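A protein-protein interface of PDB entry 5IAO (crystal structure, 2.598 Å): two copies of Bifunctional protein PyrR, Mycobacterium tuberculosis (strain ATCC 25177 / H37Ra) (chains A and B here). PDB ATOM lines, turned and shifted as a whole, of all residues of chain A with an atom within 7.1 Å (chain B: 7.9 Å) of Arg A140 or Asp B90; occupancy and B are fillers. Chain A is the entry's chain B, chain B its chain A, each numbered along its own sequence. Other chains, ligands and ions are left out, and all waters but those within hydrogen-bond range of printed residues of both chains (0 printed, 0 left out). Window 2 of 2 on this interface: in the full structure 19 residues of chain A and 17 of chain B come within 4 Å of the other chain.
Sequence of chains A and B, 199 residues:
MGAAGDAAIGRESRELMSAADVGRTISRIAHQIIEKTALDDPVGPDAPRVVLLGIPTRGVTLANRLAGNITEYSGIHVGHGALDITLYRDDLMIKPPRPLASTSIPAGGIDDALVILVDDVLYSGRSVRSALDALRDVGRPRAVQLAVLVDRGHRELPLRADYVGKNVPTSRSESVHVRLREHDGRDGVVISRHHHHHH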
ATOM      1  N   ILE A 110       3.976  20.095   3.317  1.00  0.00           N
ATOM      2  CA  ILE A 110       5.068  20.173   2.353  1.00  0.00           C
ATOM      3  C   ILE A 110       4.609  20.185   0.891  1.00  0.00           C
ATOM      4  O   ILE A 110       5.438  20.173  -0.020  1.00  0.00           O
ATOM      5  CB  ILE A 110       6.050  18.990   2.535  1.00  0.00           C
ATOM      6  CG1 ILE A 110       5.350  17.656   2.249  1.00  0.00           C
ATOM      7  CG2 ILE A 110       6.672  19.018   3.928  1.00  0.00           C
ATOM      8  CD1 ILE A 110       6.284  16.472   2.209  1.00  0.00           C
ATOM      9  N   ASP A 111       3.300  20.196   0.664  1.00  0.00           N
ATOM     10  CA  ASP A 111       2.759  20.227  -0.694  1.00  0.00           C
ATOM     11  C   ASP A 111       3.198  21.497  -1.413  1.00  0.00           C
ATOM     12  O   ASP A 111       2.973  22.609  -0.924  1.00  0.00           O
ATOM     13  CB  ASP A 111       1.237  20.133  -0.680  1.00  0.00           C
ATOM     14  CG  ASP A 111       0.741  18.754  -0.299  1.00  0.00           C
ATOM     15  OD1 ASP A 111       1.482  17.773  -0.513  1.00  0.00           O
ATOM     16  OD2 ASP A 111      -0.392  18.654   0.219  1.00  0.00           O
ATOM     17  N   ASP A 112       3.839  21.325  -2.565  1.00  0.00           N
ATOM     18  CA  ASP A 112       4.325  22.449  -3.366  1.00  0.00           C
ATOM     19  C   ASP A 112       5.369  23.273  -2.620  1.00  0.00           C
ATOM     20  O   ASP A 112       5.601  24.432  -2.950  1.00  0.00           O
ATOM     21  CB  ASP A 112       3.166  23.355  -3.788  1.00  0.00           C
ATOM     22  CG  ASP A 112       3.510  24.220  -4.983  1.00  0.00           C
ATOM     23  OD1 ASP A 112       4.206  23.722  -5.897  1.00  0.00           O
ATOM     24  OD2 ASP A 112       3.098  25.401  -4.999  1.00  0.00           O
ATOM     25  N   ALA A 113       5.997  22.674  -1.617  1.00  0.00           N
ATOM     26  CA  ALA A 113       7.080  23.344  -0.911  1.00  0.00           C
ATOM     27  C   ALA A 113       8.431  22.912  -1.467  1.00  0.00           C
ATOM     28  O   ALA A 113       8.534  21.892  -2.155  1.00  0.00           O
ATOM     29  CB  ALA A 113       7.005  23.046   0.568  1.00  0.00           C
ATOM     30  N   VAL A 115      11.442  21.311  -0.127  1.00  0.00           N
ATOM     31  CA  VAL A 115      11.886  20.607   1.068  1.00  0.00           C
ATOM     32  C   VAL A 115      13.385  20.354   1.030  1.00  0.00           C
ATOM     33  O   VAL A 115      13.913  19.819   0.052  1.00  0.00           O
ATOM     34  CB  VAL A 115      11.156  19.250   1.251  1.00  0.00           C
ATOM     35  CG1 VAL A 115      11.784  18.449   2.387  1.00  0.00           C
ATOM     36  CG2 VAL A 115       9.673  19.464   1.506  1.00  0.00           C
ATOM     37  N   LEU A 135       9.103  10.623   2.651  1.00  0.00           N
ATOM     38  CA  LEU A 135       8.598  11.934   2.277  1.00  0.00           C
ATOM     39  C   LEU A 135       7.374  11.795   1.387  1.00  0.00           C
ATOM     40  O   LEU A 135       6.464  12.626   1.411  1.00  0.00           O
ATOM     41  CB  LEU A 135       9.694  12.735   1.569  1.00  0.00           C
ATOM     42  CG  LEU A 135       9.534  14.243   1.428  1.00  0.00           C
ATOM     43  CD1 LEU A 135       9.191  14.880   2.755  1.00  0.00           C
ATOM     44  CD2 LEU A 135      10.830  14.819   0.882  1.00  0.00           C
ATOM     45  N   ARG A 136       7.344  10.720   0.613  1.00  0.00           N
ATOM     46  CA  ARG A 136       6.287  10.543  -0.360  1.00  0.00           C
ATOM     47  C   ARG A 136       4.989  10.054   0.290  1.00  0.00           C
ATOM     48  O   ARG A 136       3.925  10.133  -0.309  1.00  0.00           O
ATOM     49  CB  ARG A 136       6.769   9.574  -1.448  1.00  0.00           C
ATOM     50  CG  ARG A 136       5.814   9.383  -2.604  1.00  0.00           C
ATOM     51  CD  ARG A 136       6.486   8.662  -3.766  1.00  0.00           C
ATOM     52  NE  ARG A 136       7.164   7.437  -3.352  1.00  0.00           N
ATOM     53  CZ  ARG A 136       8.066   6.804  -4.097  1.00  0.00           C
ATOM     54  NH1 ARG A 136       8.385   7.280  -5.295  1.00  0.00           N
ATOM     55  NH2 ARG A 136       8.640   5.694  -3.650  1.00  0.00           N
ATOM     56  N   VAL A 138       4.048  11.632   2.930  1.00  0.00           N
ATOM     57  CA  VAL A 138       3.693  12.846   3.662  1.00  0.00           C
ATOM     58  C   VAL A 138       3.004  13.868   2.760  1.00  0.00           C
ATOM     59  O   VAL A 138       2.059  14.541   3.166  1.00  0.00           O
ATOM     60  CB  VAL A 138       4.933  13.504   4.292  1.00  0.00           C
ATOM     61  CG1 VAL A 138       4.580  14.881   4.841  1.00  0.00           C
ATOM     62  CG2 VAL A 138       5.525  12.610   5.385  1.00  0.00           C
ATOM     63  N   GLY A 139       3.495  13.988   1.535  1.00  0.00           N
ATOM     64  CA  GLY A 139       2.948  14.947   0.599  1.00  0.00           C
ATOM     65  C   GLY A 139       3.754  14.995  -0.682  1.00  0.00           C
ATOM     66  O   GLY A 139       4.625  14.157  -0.914  1.00  0.00           O
ATOM     67  N   ARG A 140       3.463  15.992  -1.505  1.00  0.00           N
ATOM     68  CA  ARG A 140       4.121  16.149  -2.787  1.00  0.00           C
ATOM     69  C   ARG A 140       4.804  17.504  -2.879  1.00  0.00           C
ATOM     70  O   ARG A 140       4.182  18.486  -3.281  1.00  0.00           O
ATOM     71  CB  ARG A 140       3.110  15.997  -3.923  1.00  0.00           C
ATOM     72  CG  ARG A 140       2.418  14.650  -3.949  1.00  0.00           C
ATOM     73  CD  ARG A 140       1.449  14.557  -5.113  1.00  0.00           C
ATOM     74  NE  ARG A 140       2.160  14.476  -6.385  1.00  0.00           N
ATOM     75  CZ  ARG A 140       2.632  13.350  -6.908  1.00  0.00           C
ATOM     76  NH1 ARG A 140       2.463  12.198  -6.270  1.00  0.00           N
ATOM     77  NH2 ARG A 140       3.273  13.375  -8.070  1.00  0.00           N
ATOM     78  N   PRO A 141       6.084  17.569  -2.491  1.00  0.00           N
ATOM     79  CA  PRO A 141       6.831  18.825  -2.596  1.00  0.00           C
ATOM     80  C   PRO A 141       7.091  19.236  -4.044  1.00  0.00           C
ATOM     81  O   PRO A 141       7.065  18.398  -4.945  1.00  0.00           O
ATOM     82  CB  PRO A 141       8.140  18.516  -1.863  1.00  0.00           C
ATOM     83  CG  PRO A 141       8.268  17.050  -1.899  1.00  0.00           C
ATOM     84  CD  PRO A 141       6.873  16.512  -1.842  1.00  0.00           C
ATOM     85  N   ARG A 142       7.336  20.525  -4.256  1.00  0.00           N
ATOM     86  CA  ARG A 142       7.708  21.026  -5.569  1.00  0.00           C
ATOM     87  C   ARG A 142       9.099  20.522  -5.931  1.00  0.00           C
ATOM     88  O   ARG A 142       9.367  20.180  -7.082  1.00  0.00           O
ATOM     89  CB  ARG A 142       7.668  22.554  -5.604  1.00  0.00           C
ATOM     90  CG  ARG A 142       7.892  23.130  -6.989  1.00  0.00           C
ATOM     91  CD  ARG A 142       7.886  24.645  -6.968  1.00  0.00           C
ATOM     92  NE  ARG A 142       6.622  25.190  -6.483  1.00  0.00           N
ATOM     93  CZ  ARG A 142       6.360  26.489  -6.395  1.00  0.00           C
ATOM     94  NH1 ARG A 142       7.274  27.373  -6.767  1.00  0.00           N
ATOM     95  NH2 ARG A 142       5.186  26.906  -5.944  1.00  0.00           N
ATOM     96  N   ALA A 143       9.972  20.469  -4.929  1.00  0.00           N
ATOM     97  CA  ALA A 143      11.330  19.964  -5.101  1.00  0.00           C
ATOM     98  C   ALA A 143      11.927  19.531  -3.764  1.00  0.00           C
ATOM     99  O   ALA A 143      11.482  19.973  -2.698  1.00  0.00           O
ATOM    100  CB  ALA A 143      12.217  21.022  -5.749  1.00  0.00           C
ATOM    101  N   ILE B  85       9.605   1.651 -16.245  1.00  0.00           N
ATOM    102  CA  ILE B  85       9.241   2.395 -15.046  1.00  0.00           C
ATOM    103  C   ILE B  85       7.799   2.881 -15.094  1.00  0.00           C
ATOM    104  O   ILE B  85       7.417   3.800 -14.368  1.00  0.00           O
ATOM    105  CB  ILE B  85      10.141   3.620 -14.849  1.00  0.00           C
ATOM    106  CG1 ILE B  85       9.987   4.571 -16.042  1.00  0.00           C
ATOM    107  CG2 ILE B  85      11.582   3.202 -14.652  1.00  0.00           C
ATOM    108  CD1 ILE B  85      10.579   5.936 -15.806  1.00  0.00           C
ATOM    109  N   THR B  86       7.004   2.273 -15.964  1.00  0.00           N
ATOM    110  CA  THR B  86       5.630   2.710 -16.165  1.00  0.00           C
ATOM    111  C   THR B  86       4.803   2.620 -14.888  1.00  0.00           C
ATOM    112  O   THR B  86       4.057   3.538 -14.557  1.00  0.00           O
ATOM    113  CB  THR B  86       4.942   1.878 -17.256  1.00  0.00           C
ATOM    114  OG1 THR B  86       5.788   1.804 -18.410  1.00  0.00           O
ATOM    115  CG2 THR B  86       3.616   2.499 -17.629  1.00  0.00           C
ATOM    116  N   LEU B  87       4.962   1.514 -14.169  1.00  0.00           N
ATOM    117  CA  LEU B  87       4.180   1.245 -12.970  1.00  0.00           C
ATOM    118  C   LEU B  87       4.847   1.835 -11.737  1.00  0.00           C
ATOM    119  O   LEU B  87       4.521   1.468 -10.604  1.00  0.00           O
ATOM    120  CB  LEU B  87       4.017  -0.267 -12.787  1.00  0.00           C
ATOM    121  CG  LEU B  87       3.454  -1.031 -13.984  1.00  0.00           C
ATOM    122  CD1 LEU B  87       3.459  -2.521 -13.721  1.00  0.00           C
ATOM    123  CD2 LEU B  87       2.057  -0.549 -14.301  1.00  0.00           C
ATOM    124  N   TYR B  88       5.758   2.774 -11.959  1.00  0.00           N
ATOM    125  CA  TYR B  88       6.584   3.288 -10.876  1.00  0.00           C
ATOM    126  C   TYR B  88       6.612   4.809 -10.871  1.00  0.00           C
ATOM    127  O   TYR B  88       7.520   5.421 -10.310  1.00  0.00           O
ATOM    128  CB  TYR B  88       8.004   2.733 -10.990  1.00  0.00           C
ATOM    129  CG  TYR B  88       8.098   1.241 -10.767  1.00  0.00           C
ATOM    130  CD1 TYR B  88       8.055   0.352 -11.841  1.00  0.00           C
ATOM    131  CD2 TYR B  88       8.224   0.715  -9.486  1.00  0.00           C
ATOM    132  CE1 TYR B  88       8.144  -1.022 -11.642  1.00  0.00           C
ATOM    133  CE2 TYR B  88       8.309  -0.657  -9.276  1.00  0.00           C
ATOM    134  CZ  TYR B  88       8.267  -1.516 -10.356  1.00  0.00           C
ATOM    135  OH  TYR B  88       8.352  -2.869 -10.150  1.00  0.00           O
ATOM    136  N   ARG B  89       5.605   5.416 -11.486  1.00  0.00           N
ATOM    137  CA  ARG B  89       5.535   6.864 -11.558  1.00  0.00           C
ATOM    138  C   ARG B  89       4.528   7.378 -10.536  1.00  0.00           C
ATOM    139  O   ARG B  89       3.928   6.594  -9.799  1.00  0.00           O
ATOM    140  CB  ARG B  89       5.150   7.313 -12.966  1.00  0.00           C
ATOM    141  CG  ARG B  89       6.150   6.907 -14.039  1.00  0.00           C
ATOM    142  CD  ARG B  89       5.706   7.395 -15.406  1.00  0.00           C
ATOM    143  NE  ARG B  89       6.609   6.977 -16.476  1.00  0.00           N
ATOM    144  CZ  ARG B  89       7.787   7.535 -16.729  1.00  0.00           C
ATOM    145  NH1 ARG B  89       8.228   8.538 -15.975  1.00  0.00           N
ATOM    146  NH2 ARG B  89       8.532   7.084 -17.732  1.00  0.00           N
ATOM    147  N   ASP B  90       4.338   8.693 -10.499  1.00  0.00           N
ATOM    148  CA  ASP B  90       3.420   9.313  -9.548  1.00  0.00           C
ATOM    149  C   ASP B  90       2.080   9.680 -10.188  1.00  0.00           C
ATOM    150  O   ASP B  90       1.935  10.740 -10.798  1.00  0.00           O
ATOM    151  CB  ASP B  90       4.071  10.554  -8.939  1.00  0.00           C
ATOM    152  CG  ASP B  90       5.440  10.258  -8.345  1.00  0.00           C
ATOM    153  OD1 ASP B  90       5.586   9.209  -7.677  1.00  0.00           O
ATOM    154  OD2 ASP B  90       6.369  11.072  -8.548  1.00  0.00           O
ATOM    155  N   ARG B 126      12.839  12.751 -11.804  1.00  0.00           N
ATOM    156  CA  ARG B 126      11.766  11.868 -11.360  1.00  0.00           C
ATOM    157  C   ARG B 126      11.747  10.524 -12.082  1.00  0.00           C
ATOM    158  O   ARG B 126      11.444   9.501 -11.468  1.00  0.00           O
ATOM    159  CB  ARG B 126      10.416  12.566 -11.517  1.00  0.00           C
ATOM    160  CG  ARG B 126      10.278  13.768 -10.613  1.00  0.00           C
ATOM    161  CD  ARG B 126       8.868  14.319 -10.581  1.00  0.00           C
ATOM    162  NE  ARG B 126       8.798  15.517  -9.743  1.00  0.00           N
ATOM    163  CZ  ARG B 126       8.814  15.515  -8.413  1.00  0.00           C
ATOM    164  NH1 ARG B 126       8.875  14.367  -7.742  1.00  0.00           N
ATOM    165  NH2 ARG B 126       8.755  16.666  -7.752  1.00  0.00           N
ATOM    166  N   SER B 127      12.114  10.509 -13.363  1.00  0.00           N
ATOM    167  CA  SER B 127      12.177   9.252 -14.112  1.00  0.00           C
ATOM    168  C   SER B 127      13.223   8.313 -13.530  1.00  0.00           C
ATOM    169  O   SER B 127      12.986   7.112 -13.388  1.00  0.00           O
ATOM    170  CB  SER B 127      12.483   9.512 -15.586  1.00  0.00           C
ATOM    171  OG  SER B 127      11.382  10.115 -16.235  1.00  0.00           O
ATOM    172  N   ARG B 129      14.338   8.335 -10.436  1.00  0.00           N
ATOM    173  CA  ARG B 129      13.872   7.855  -9.136  1.00  0.00           C
ATOM    174  C   ARG B 129      12.925   6.668  -9.333  1.00  0.00           C
ATOM    175  O   ARG B 129      12.980   5.693  -8.581  1.00  0.00           O
ATOM    176  CB  ARG B 129      13.178   8.969  -8.351  1.00  0.00           C
ATOM    177  CG  ARG B 129      12.597   8.513  -7.025  1.00  0.00           C
ATOM    178  CD  ARG B 129      11.124   8.833  -6.918  1.00  0.00           C
ATOM    179  NE  ARG B 129      10.793   9.496  -5.659  1.00  0.00           N
ATOM    180  CZ  ARG B 129      10.877   8.915  -4.468  1.00  0.00           C
ATOM    181  NH1 ARG B 129      11.297   7.659  -4.373  1.00  0.00           N
ATOM    182  NH2 ARG B 129      10.553   9.591  -3.375  1.00  0.00           N
ATOM    183  N   SER B 130      12.066   6.753 -10.349  1.00  0.00           N
ATOM    184  CA  SER B 130      11.185   5.640 -10.709  1.00  0.00           C
ATOM    185  C   SER B 130      12.004   4.401 -11.051  1.00  0.00           C
ATOM    186  O   SER B 130      11.648   3.289 -10.672  1.00  0.00           O
ATOM    187  CB  SER B 130      10.290   5.999 -11.902  1.00  0.00           C
ATOM    188  OG  SER B 130       9.422   7.076 -11.610  1.00  0.00           O
ATOM    189  N   ASP B 133      13.171   2.760  -7.955  1.00  0.00           N
ATOM    190  CA  ASP B 133      12.103   1.970  -7.355  1.00  0.00           C
ATOM    191  C   ASP B 133      11.904   0.675  -8.111  1.00  0.00           C
ATOM    192  O   ASP B 133      11.863  -0.405  -7.520  1.00  0.00           O
ATOM    193  CB  ASP B 133      10.792   2.752  -7.321  1.00  0.00           C
ATOM    194  CG  ASP B 133      10.801   3.838  -6.276  1.00  0.00           C
ATOM    195  OD1 ASP B 133      11.663   3.769  -5.375  1.00  0.00           O
ATOM    196  OD2 ASP B 133       9.937   4.739  -6.338  1.00  0.00           O
ATOM    197  N   LEU B 157      14.921  16.607  -7.328  1.00  0.00           N
ATOM    198  CA  LEU B 157      15.365  15.621  -6.349  1.00  0.00           C
ATOM    199  C   LEU B 157      16.884  15.687  -6.241  1.00  0.00           C
ATOM    200  O   LEU B 157      17.550  16.134  -7.174  1.00  0.00           O
ATOM    201  CB  LEU B 157      14.918  14.205  -6.748  1.00  0.00           C
ATOM    202  CG  LEU B 157      13.416  13.916  -6.831  1.00  0.00           C
ATOM    203  CD1 LEU B 157      13.153  12.594  -7.526  1.00  0.00           C
ATOM    204  CD2 LEU B 157      12.794  13.910  -5.444  1.00  0.00           C
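The side-chain carboxylate (OD2) of Asp B90 is in salt-bridge range of the guanidinium group (NH2) of Arg A140 (3.9 Å).
The side-chain carboxylate of Asp B133 is in salt-bridge range of the guanidinium group of Arg A136, 3.1 Å away.
The guanidinium group of Arg B129 sits close to the guanidinium group of Arg A136, at 3.1 Å.
OD2 of Asp A112 is in salt-bridge range of NH2 of Arg A142, 2.7 Å away.
The side-chain carboxylate (OD2) of Asp B133 lies within salt-bridge range of the guanidinium group (NH1) of Arg B129.
The backbone carbonyl oxygen (O) of Arg B126 sits at hydrogen-bond distance from the side-chain hydroxyl (OG) of Ser B130 (3.2 Å).
The side-chain carboxylate (OD1) of Asp A111 sits at hydrogen-bond distance from the backbone NH (N) of Arg A140, at 2.8 Å.
The backbone NH of Asp A112 sits at hydrogen-bond distance from the backbone carbonyl oxygen of Arg A140 (2.9 Å).
The backbone carbonyl oxygen (O) of Ala A113 is in hydrogen-bond range of the backbone NH (N) of Arg A142.
Pro A141 touches Arg B126.
Arg A142 touches Arg B126.
Printed residues of chain B within 4 Å of Arg A136: Arg B129 and Asp B133.
No residue of chain B comes within 4 Å of Gly A139.
Arg A140 touches just one residue of chain B: Asp B90.
Of chain B, only Arg B126 comes within 4 Å of Pro A141.
Printed residues of chain B within 4 Å of Arg A142: Arg B126 (3.6 Å).
Of chain A, only Arg A140 comes within 4 Å of Asp B90.
Of the printed residues of chain A, Arg B129 touches Arg A136.
Of the printed residues of chain A, Asp B133 touches Arg A136.
The nearest residue of chain B that does not touch Arg A140 is Arg B126 (5.7 Å).
The nearest printed residue of chain A that does not touch Arg B129 is Leu A135 (5.9 Å).
No position is printed for both chains.
Of the 5 pairs that touch across the chains among the printed residues, none has its exchanged pair printed and touching as well.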
